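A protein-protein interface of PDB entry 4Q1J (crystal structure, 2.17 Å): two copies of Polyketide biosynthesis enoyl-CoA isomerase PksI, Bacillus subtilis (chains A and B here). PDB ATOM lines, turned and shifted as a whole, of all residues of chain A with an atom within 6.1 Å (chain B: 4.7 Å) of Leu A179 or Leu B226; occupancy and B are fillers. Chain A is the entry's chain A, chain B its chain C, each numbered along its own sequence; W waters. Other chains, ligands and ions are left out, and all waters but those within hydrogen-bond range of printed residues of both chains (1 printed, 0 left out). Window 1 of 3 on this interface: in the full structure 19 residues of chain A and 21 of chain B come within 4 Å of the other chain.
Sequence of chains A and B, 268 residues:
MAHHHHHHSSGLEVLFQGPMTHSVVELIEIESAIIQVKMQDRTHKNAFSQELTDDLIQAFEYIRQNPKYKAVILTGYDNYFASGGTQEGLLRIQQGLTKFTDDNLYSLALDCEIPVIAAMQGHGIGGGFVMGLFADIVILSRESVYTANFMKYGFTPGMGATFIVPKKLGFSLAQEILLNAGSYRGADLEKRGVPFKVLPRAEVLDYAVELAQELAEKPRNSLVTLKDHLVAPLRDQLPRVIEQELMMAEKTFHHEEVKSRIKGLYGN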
ATOM      1  N   MET A 151      -2.887  10.743 -21.451  1.00  0.00           N
ATOM      2  CA  MET A 151      -2.123  10.783 -22.695  1.00  0.00           C
ATOM      3  C   MET A 151      -0.720  11.427 -22.585  1.00  0.00           C
ATOM      4  O   MET A 151       0.188  11.091 -23.359  1.00  0.00           O
ATOM      5  CB  MET A 151      -3.011  11.404 -23.847  1.00  0.00           C
ATOM      6  CG  MET A 151      -4.135  10.450 -24.309  1.00  0.00           C
ATOM      7  SD  MET A 151      -3.510   9.433 -25.688  1.00  0.00           S
ATOM      8  CE  MET A 151      -4.083   7.855 -25.280  1.00  0.00           C
ATOM      9  N   THR A 156      -3.786   5.662 -23.116  1.00  0.00           N
ATOM     10  CA  THR A 156      -5.174   6.097 -23.446  1.00  0.00           C
ATOM     11  C   THR A 156      -5.991   6.260 -22.142  1.00  0.00           C
ATOM     12  O   THR A 156      -5.677   5.591 -21.104  1.00  0.00           O
ATOM     13  CB  THR A 156      -5.842   5.103 -24.398  1.00  0.00           C
ATOM     14  OG1 THR A 156      -5.652   3.774 -23.885  1.00  0.00           O
ATOM     15  CG2 THR A 156      -5.157   5.174 -25.819  1.00  0.00           C
ATOM     16  N   PRO A 157      -7.013   7.165 -22.154  1.00  0.00           N
ATOM     17  CA  PRO A 157      -7.708   7.401 -20.901  1.00  0.00           C
ATOM     18  C   PRO A 157      -8.421   6.132 -20.376  1.00  0.00           C
ATOM     19  O   PRO A 157      -8.914   5.298 -21.176  1.00  0.00           O
ATOM     20  CB  PRO A 157      -8.732   8.465 -21.293  1.00  0.00           C
ATOM     21  CG  PRO A 157      -8.030   9.269 -22.361  1.00  0.00           C
ATOM     22  CD  PRO A 157      -7.328   8.219 -23.169  1.00  0.00           C
ATOM     23  N   THR A 162     -13.379   8.663 -21.021  1.00  0.00           N
ATOM     24  CA  THR A 162     -13.871   8.892 -22.382  1.00  0.00           C
ATOM     25  C   THR A 162     -15.411   8.892 -22.430  1.00  0.00           C
ATOM     26  O   THR A 162     -15.999   9.216 -23.449  1.00  0.00           O
ATOM     27  CB  THR A 162     -13.343   7.875 -23.419  1.00  0.00           C
ATOM     28  OG1 THR A 162     -13.939   6.600 -23.185  1.00  0.00           O
ATOM     29  CG2 THR A 162     -11.803   7.796 -23.477  1.00  0.00           C
ATOM     30  N   ALA A 174     -14.174  17.877 -24.712  1.00  0.00           N
ATOM     31  CA  ALA A 174     -13.690  16.510 -24.485  1.00  0.00           C
ATOM     32  C   ALA A 174     -12.620  16.031 -25.466  1.00  0.00           C
ATOM     33  O   ALA A 174     -11.624  15.462 -24.976  1.00  0.00           O
ATOM     34  CB  ALA A 174     -14.843  15.507 -24.428  1.00  0.00           C
ATOM     35  N   GLN A 175     -12.769  16.247 -26.795  1.00  0.00           N
ATOM     36  CA  GLN A 175     -11.734  15.842 -27.770  1.00  0.00           C
ATOM     37  C   GLN A 175     -10.362  16.444 -27.399  1.00  0.00           C
ATOM     38  O   GLN A 175      -9.310  15.702 -27.304  1.00  0.00           O
ATOM     39  CB  GLN A 175     -12.105  16.207 -29.233  1.00  0.00           C
ATOM     40  CG  GLN A 175     -13.511  15.788 -29.600  1.00  0.00           C
ATOM     41  CD  GLN A 175     -13.717  14.345 -29.230  1.00  0.00           C
ATOM     42  OE1 GLN A 175     -13.061  13.484 -29.806  1.00  0.00           O
ATOM     43  NE2 GLN A 175     -14.557  14.067 -28.216  1.00  0.00           N
ATOM     44  N   GLU A 176     -10.357  17.763 -27.169  1.00  0.00           N
ATOM     45  CA  GLU A 176      -9.151  18.484 -26.785  1.00  0.00           C
ATOM     46  C   GLU A 176      -8.586  18.009 -25.406  1.00  0.00           C
ATOM     47  O   GLU A 176      -7.391  17.794 -25.278  1.00  0.00           O
ATOM     48  CB  GLU A 176      -9.419  19.983 -26.733  1.00  0.00           C
ATOM     49  CG  GLU A 176      -8.183  20.837 -26.591  1.00  0.00           C
ATOM     50  CD  GLU A 176      -8.593  22.305 -26.312  1.00  0.00           C
ATOM     51  OE1 GLU A 176      -9.299  22.843 -27.175  1.00  0.00           O
ATOM     52  OE2 GLU A 176      -8.262  22.919 -25.241  1.00  0.00           O
ATOM     53  N   ILE A 177      -9.434  17.934 -24.397  1.00  0.00           N
ATOM     54  CA  ILE A 177      -9.003  17.568 -23.076  1.00  0.00           C
ATOM     55  C   ILE A 177      -8.350  16.174 -23.086  1.00  0.00           C
ATOM     56  O   ILE A 177      -7.297  15.966 -22.480  1.00  0.00           O
ATOM     57  CB  ILE A 177     -10.196  17.598 -22.088  1.00  0.00           C
ATOM     58  CG1 ILE A 177     -10.510  19.052 -21.773  1.00  0.00           C
ATOM     59  CG2 ILE A 177      -9.961  16.714 -20.760  1.00  0.00           C
ATOM     60  CD1 ILE A 177     -11.808  19.261 -21.033  1.00  0.00           C
ATOM     61  N   LEU A 178      -8.959  15.260 -23.823  1.00  0.00           N
ATOM     62  CA  LEU A 178      -8.556  13.892 -23.790  1.00  0.00           C
ATOM     63  C   LEU A 178      -7.358  13.590 -24.711  1.00  0.00           C
ATOM     64  O   LEU A 178      -6.421  12.838 -24.300  1.00  0.00           O
ATOM     65  CB  LEU A 178      -9.747  12.952 -24.081  1.00  0.00           C
ATOM     66  CG  LEU A 178     -10.922  12.953 -23.098  1.00  0.00           C
ATOM     67  CD1 LEU A 178     -12.114  12.132 -23.642  1.00  0.00           C
ATOM     68  CD2 LEU A 178     -10.423  12.438 -21.732  1.00  0.00           C
ATOM     69  N   LEU A 179      -7.419  14.086 -25.945  1.00  0.00           N
ATOM     70  CA  LEU A 179      -6.346  13.882 -26.936  1.00  0.00           C
ATOM     71  C   LEU A 179      -5.046  14.539 -26.472  1.00  0.00           C
ATOM     72  O   LEU A 179      -3.958  13.926 -26.547  1.00  0.00           O
ATOM     73  CB  LEU A 179      -6.700  14.435 -28.338  1.00  0.00           C
ATOM     74  CG  LEU A 179      -7.704  13.561 -29.133  1.00  0.00           C
ATOM     75  CD1 LEU A 179      -8.395  14.242 -30.295  1.00  0.00           C
ATOM     76  CD2 LEU A 179      -7.039  12.297 -29.628  1.00  0.00           C
ATOM     77  N   ASN A 180      -5.149  15.755 -25.949  1.00  0.00           N
ATOM     78  CA  ASN A 180      -3.925  16.479 -25.743  1.00  0.00           C
ATOM     79  C   ASN A 180      -3.447  16.434 -24.262  1.00  0.00           C
ATOM     80  O   ASN A 180      -2.321  16.872 -23.977  1.00  0.00           O
ATOM     81  CB  ASN A 180      -4.070  17.919 -26.256  1.00  0.00           C
ATOM     82  CG  ASN A 180      -2.716  18.640 -26.362  1.00  0.00           C
ATOM     83  OD1 ASN A 180      -2.575  19.819 -25.960  1.00  0.00           O
ATOM     84  ND2 ASN A 180      -1.704  17.926 -26.849  1.00  0.00           N
ATOM     85  N   ALA A 181      -4.309  15.988 -23.331  1.00  0.00           N
ATOM     86  CA  ALA A 181      -3.931  15.852 -21.952  1.00  0.00           C
ATOM     87  C   ALA A 181      -3.422  17.159 -21.334  1.00  0.00           C
ATOM     88  O   ALA A 181      -2.571  17.141 -20.412  1.00  0.00           O
ATOM     89  CB  ALA A 181      -2.875  14.711 -21.809  1.00  0.00           C
ATOM     90  N   MET A 248      -8.517  -0.441 -25.529  1.00  0.00           N
ATOM     91  CA  MET A 248      -7.566   0.617 -25.847  1.00  0.00           C
ATOM     92  C   MET A 248      -6.262   0.441 -25.035  1.00  0.00           C
ATOM     93  O   MET A 248      -5.172   0.512 -25.569  1.00  0.00           O
ATOM     94  CB  MET A 248      -8.173   2.012 -25.600  1.00  0.00           C
ATOM     95  CG  MET A 248      -9.185   2.495 -26.671  1.00  0.00           C
ATOM     96  SD  MET A 248      -9.393   4.272 -26.401  1.00  0.00           S
ATOM     97  CE  MET A 248      -7.862   4.723 -27.044  1.00  0.00           C
ATOM     98  N   PRO B 115      -5.295  13.196 -35.486  1.00  0.00           N
ATOM     99  CA  PRO B 115      -6.068  14.368 -35.152  1.00  0.00           C
ATOM    100  C   PRO B 115      -5.870  15.449 -36.185  1.00  0.00           C
ATOM    101  O   PRO B 115      -4.767  15.592 -36.744  1.00  0.00           O
ATOM    102  CB  PRO B 115      -5.470  14.800 -33.829  1.00  0.00           C
ATOM    103  CG  PRO B 115      -4.981  13.520 -33.249  1.00  0.00           C
ATOM    104  CD  PRO B 115      -4.384  12.819 -34.414  1.00  0.00           C
ATOM    105  N   ASP B 136     -11.060  17.348 -35.320  1.00  0.00           N
ATOM    106  CA  ASP B 136     -11.063  17.041 -33.893  1.00  0.00           C
ATOM    107  C   ASP B 136     -10.984  18.302 -33.027  1.00  0.00           C
ATOM    108  O   ASP B 136     -11.488  18.321 -31.904  1.00  0.00           O
ATOM    109  CB  ASP B 136      -9.910  16.095 -33.548  1.00  0.00           C
ATOM    110  CG  ASP B 136      -9.890  14.858 -34.425  1.00  0.00           C
ATOM    111  OD1 ASP B 136     -10.669  13.922 -34.153  1.00  0.00           O
ATOM    112  OD2 ASP B 136      -9.093  14.824 -35.387  1.00  0.00           O
ATOM    113  N   LEU B 215       0.393  17.954 -29.395  1.00  0.00           N
ATOM    114  CA  LEU B 215      -0.203  16.695 -29.838  1.00  0.00           C
ATOM    115  C   LEU B 215       0.891  15.756 -30.324  1.00  0.00           C
ATOM    116  O   LEU B 215       0.799  14.550 -30.100  1.00  0.00           O
ATOM    117  CB  LEU B 215      -1.247  16.896 -30.970  1.00  0.00           C
ATOM    118  CG  LEU B 215      -2.592  17.529 -30.541  1.00  0.00           C
ATOM    119  CD1 LEU B 215      -3.491  17.935 -31.743  1.00  0.00           C
ATOM    120  CD2 LEU B 215      -3.277  16.572 -29.581  1.00  0.00           C
ATOM    121  N   LYS B 218       2.894  12.990 -28.198  1.00  0.00           N
ATOM    122  CA  LYS B 218       2.301  11.695 -27.883  1.00  0.00           C
ATOM    123  C   LYS B 218       2.737  10.607 -28.921  1.00  0.00           C
ATOM    124  O   LYS B 218       2.981  10.908 -30.096  1.00  0.00           O
ATOM    125  CB  LYS B 218       0.760  11.876 -27.908  1.00  0.00           C
ATOM    126  CG  LYS B 218       0.113  12.428 -26.624  1.00  0.00           C
ATOM    127  CD  LYS B 218       0.585  13.820 -26.252  1.00  0.00           C
ATOM    128  CE  LYS B 218      -0.415  14.597 -25.419  1.00  0.00           C
ATOM    129  NZ  LYS B 218       0.016  16.042 -25.362  1.00  0.00           N
ATOM    130  N   SER B 222      -0.967   5.891 -29.839  1.00  0.00           N
ATOM    131  CA  SER B 222      -1.929   6.275 -28.797  1.00  0.00           C
ATOM    132  C   SER B 222      -2.920   7.311 -29.364  1.00  0.00           C
ATOM    133  O   SER B 222      -4.098   7.255 -29.029  1.00  0.00           O
ATOM    134  CB  SER B 222      -1.239   6.849 -27.564  1.00  0.00           C
ATOM    135  OG  SER B 222      -0.418   5.873 -26.947  1.00  0.00           O
ATOM    136  N   LEU B 223      -2.441   8.199 -30.232  1.00  0.00           N
ATOM    137  CA  LEU B 223      -3.298   9.222 -30.855  1.00  0.00           C
ATOM    138  C   LEU B 223      -4.359   8.649 -31.798  1.00  0.00           C
ATOM    139  O   LEU B 223      -5.515   9.105 -31.836  1.00  0.00           O
ATOM    140  CB  LEU B 223      -2.442  10.226 -31.624  1.00  0.00           C
ATOM    141  CG  LEU B 223      -1.573  11.258 -30.874  1.00  0.00           C
ATOM    142  CD1 LEU B 223      -0.775  11.971 -31.972  1.00  0.00           C
ATOM    143  CD2 LEU B 223      -2.389  12.299 -30.056  1.00  0.00           C
ATOM    144  N   VAL B 224      -3.956   7.659 -32.596  1.00  0.00           N
ATOM    145  CA  VAL B 224      -4.866   6.997 -33.531  1.00  0.00           C
ATOM    146  C   VAL B 224      -5.850   6.105 -32.749  1.00  0.00           C
ATOM    147  O   VAL B 224      -7.073   6.159 -32.959  1.00  0.00           O
ATOM    148  CB  VAL B 224      -4.082   6.238 -34.647  1.00  0.00           C
ATOM    149  CG1 VAL B 224      -5.051   5.384 -35.512  1.00  0.00           C
ATOM    150  CG2 VAL B 224      -3.273   7.250 -35.471  1.00  0.00           C
ATOM    151  N   THR B 225      -5.324   5.295 -31.833  1.00  0.00           N
ATOM    152  CA  THR B 225      -6.177   4.496 -30.990  1.00  0.00           C
ATOM    153  C   THR B 225      -7.235   5.334 -30.218  1.00  0.00           C
ATOM    154  O   THR B 225      -8.386   4.906 -30.099  1.00  0.00           O
ATOM    155  CB  THR B 225      -5.354   3.672 -29.978  1.00  0.00           C
ATOM    156  OG1 THR B 225      -4.494   2.816 -30.727  1.00  0.00           O
ATOM    157  CG2 THR B 225      -6.286   2.763 -29.083  1.00  0.00           C
ATOM    158  N   LEU B 226      -6.843   6.478 -29.672  1.00  0.00           N
ATOM    159  CA  LEU B 226      -7.825   7.261 -29.001  1.00  0.00           C
ATOM    160  C   LEU B 226      -8.778   7.996 -29.993  1.00  0.00           C
ATOM    161  O   LEU B 226      -9.986   7.963 -29.735  1.00  0.00           O
ATOM    162  CB  LEU B 226      -7.177   8.212 -27.988  1.00  0.00           C
ATOM    163  CG  LEU B 226      -8.157   9.117 -27.261  1.00  0.00           C
ATOM    164  CD1 LEU B 226      -9.131   8.351 -26.404  1.00  0.00           C
ATOM    165  CD2 LEU B 226      -7.358  10.121 -26.454  1.00  0.00           C
ATOM    166  N   LYS B 227      -8.286   8.553 -31.121  1.00  0.00           N
ATOM    167  CA  LYS B 227      -9.230   9.186 -32.115  1.00  0.00           C
ATOM    168  C   LYS B 227     -10.265   8.134 -32.577  1.00  0.00           C
ATOM    169  O   LYS B 227     -11.464   8.413 -32.541  1.00  0.00           O
ATOM    170  CB  LYS B 227      -8.556   9.920 -33.314  1.00  0.00           C
ATOM    171  CG  LYS B 227      -9.570  10.637 -34.237  1.00  0.00           C
ATOM    172  CD  LYS B 227      -8.922  11.307 -35.520  1.00  0.00           C
ATOM    173  CE  LYS B 227     -10.011  11.818 -36.447  1.00  0.00           C
ATOM    174  NZ  LYS B 227      -9.538  12.856 -37.454  1.00  0.00           N
ATOM    175  N   ASP B 228      -9.805   6.941 -32.973  1.00  0.00           N
ATOM    176  CA  ASP B 228     -10.748   5.831 -33.355  1.00  0.00           C
ATOM    177  C   ASP B 228     -11.890   5.641 -32.377  1.00  0.00           C
ATOM    178  O   ASP B 228     -13.052   5.497 -32.757  1.00  0.00           O
ATOM    179  CB  ASP B 228     -10.038   4.497 -33.425  1.00  0.00           C
ATOM    180  CG  ASP B 228      -9.245   4.316 -34.715  1.00  0.00           C
ATOM    181  OD1 ASP B 228      -9.335   5.153 -35.587  1.00  0.00           O
ATOM    182  OD2 ASP B 228      -8.439   3.342 -34.788  1.00  0.00           O
ATOM    183  N   HIS B 229     -11.528   5.585 -31.093  1.00  0.00           N
ATOM    184  CA  HIS B 229     -12.473   5.331 -30.054  1.00  0.00           C
ATOM    185  C   HIS B 229     -13.352   6.599 -29.839  1.00  0.00           C
ATOM    186  O   HIS B 229     -14.560   6.531 -29.881  1.00  0.00           O
ATOM    187  CB  HIS B 229     -11.710   4.932 -28.789  1.00  0.00           C
ATOM    188  CG  HIS B 229     -12.575   4.923 -27.580  1.00  0.00           C
ATOM    189  ND1 HIS B 229     -13.521   3.949 -27.364  1.00  0.00           N
ATOM    190  CD2 HIS B 229     -12.731   5.837 -26.591  1.00  0.00           C
ATOM    191  CE1 HIS B 229     -14.208   4.242 -26.274  1.00  0.00           C
ATOM    192  NE2 HIS B 229     -13.731   5.367 -25.762  1.00  0.00           N
ATOM    193  N   LEU B 230     -12.773   7.779 -29.700  1.00  0.00           N
ATOM    194  CA  LEU B 230     -13.636   8.999 -29.591  1.00  0.00           C
ATOM    195  C   LEU B 230     -14.554   9.236 -30.777  1.00  0.00           C
ATOM    196  O   LEU B 230     -15.648   9.778 -30.628  1.00  0.00           O
ATOM    197  CB  LEU B 230     -12.799  10.282 -29.407  1.00  0.00           C
ATOM    198  CG  LEU B 230     -12.003  10.289 -28.104  1.00  0.00           C
ATOM    199  CD1 LEU B 230     -11.083  11.516 -28.006  1.00  0.00           C
ATOM    200  CD2 LEU B 230     -12.963  10.121 -26.920  1.00  0.00           C
HETATM  201  O   HOH W   1     -10.957  12.698 -31.896  1.00  0.00           O
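O of Asn A180 lies within hydrogen-bond range of NZ of Lys B218 (2.8 Å). NE2 of His B229 is in hydrogen-bond range of OG1 of Thr A162 (2.9 Å). The side-chain amide nitrogen of Asn A180 lies close to the backbone NH of Leu B215 (3.3 Å).
OD2 of Asp B136 is in salt-bridge range of NZ of Lys B227 (2.9 Å).
Met A151 touches Ser B222 (CE to CB, 3.8 Å). Thr A156 touches Ser B222 (CG2 to O, 3.97 Å). Gln A175 touches Leu B230. Leu A178 touches Leu B226 (O to CD2, 3.6 Å). CD1 of Leu A178 touches CD2 of Leu B230, at 3.9 Å. Leu A179 touches Lys B218 (O to CE, 3.8 Å). Leu B226 touches Leu A179 (CD2 to CD2, 3.9 Å). Met A248 touches Thr B225. Met A248 touches Leu B226. CB of His B229 touches SD of Met A248, 3.4 Å away.
Printed residues of chain B within 4 Å of Met A151: Lys B218 (3.5 Å), Ser B222 (3.8 Å) and Leu B226 (3.9 Å). Of the printed residues of chain B, Thr A156 touches Ser B222. Leu A179 touches two residues of chain B. Pro B115 touches none of the printed residues of chain A. Of the printed residues of chain A, Leu B215 touches Asn A180. Leu B223 touches none of the printed residues of chain A. Of the printed residues of chain A, Leu B226 touches Met A151, Pro A157, Leu A178, Leu A179 and Met A248. The nearest printed residue of chain A that does not touch Leu B226 is Thr A162 (4.002 Å).
Of the 13 printed residues of chain B, 8 touch a printed residue of chain A. Hydrophobic or aromatic side chains of chain B that line the printed part of chain A: Leu B215, Leu B226, His B229 and Leu B230. Hydrophobic or aromatic side chains of chain A that line the printed part of chain B: Met A151, Pro A157, Leu A178, Leu A179 and Met A248. Among the printed residues, 17 pairs touch across the chains. Among the printed residues, no Asp or Glu carboxylate lies within 4 Å of a Lys or Arg side-chain nitrogen of the other chain.
No position is printed for both chains. Of the 17 pairs that touch across the chains among the printed residues, none has its exchanged pair printed and touching as well.
Water W1 lies within hydrogen-bond range of OD1 of Asp B136 (2.6 Å) and OE1 of Gln A175 (3.1 Å).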
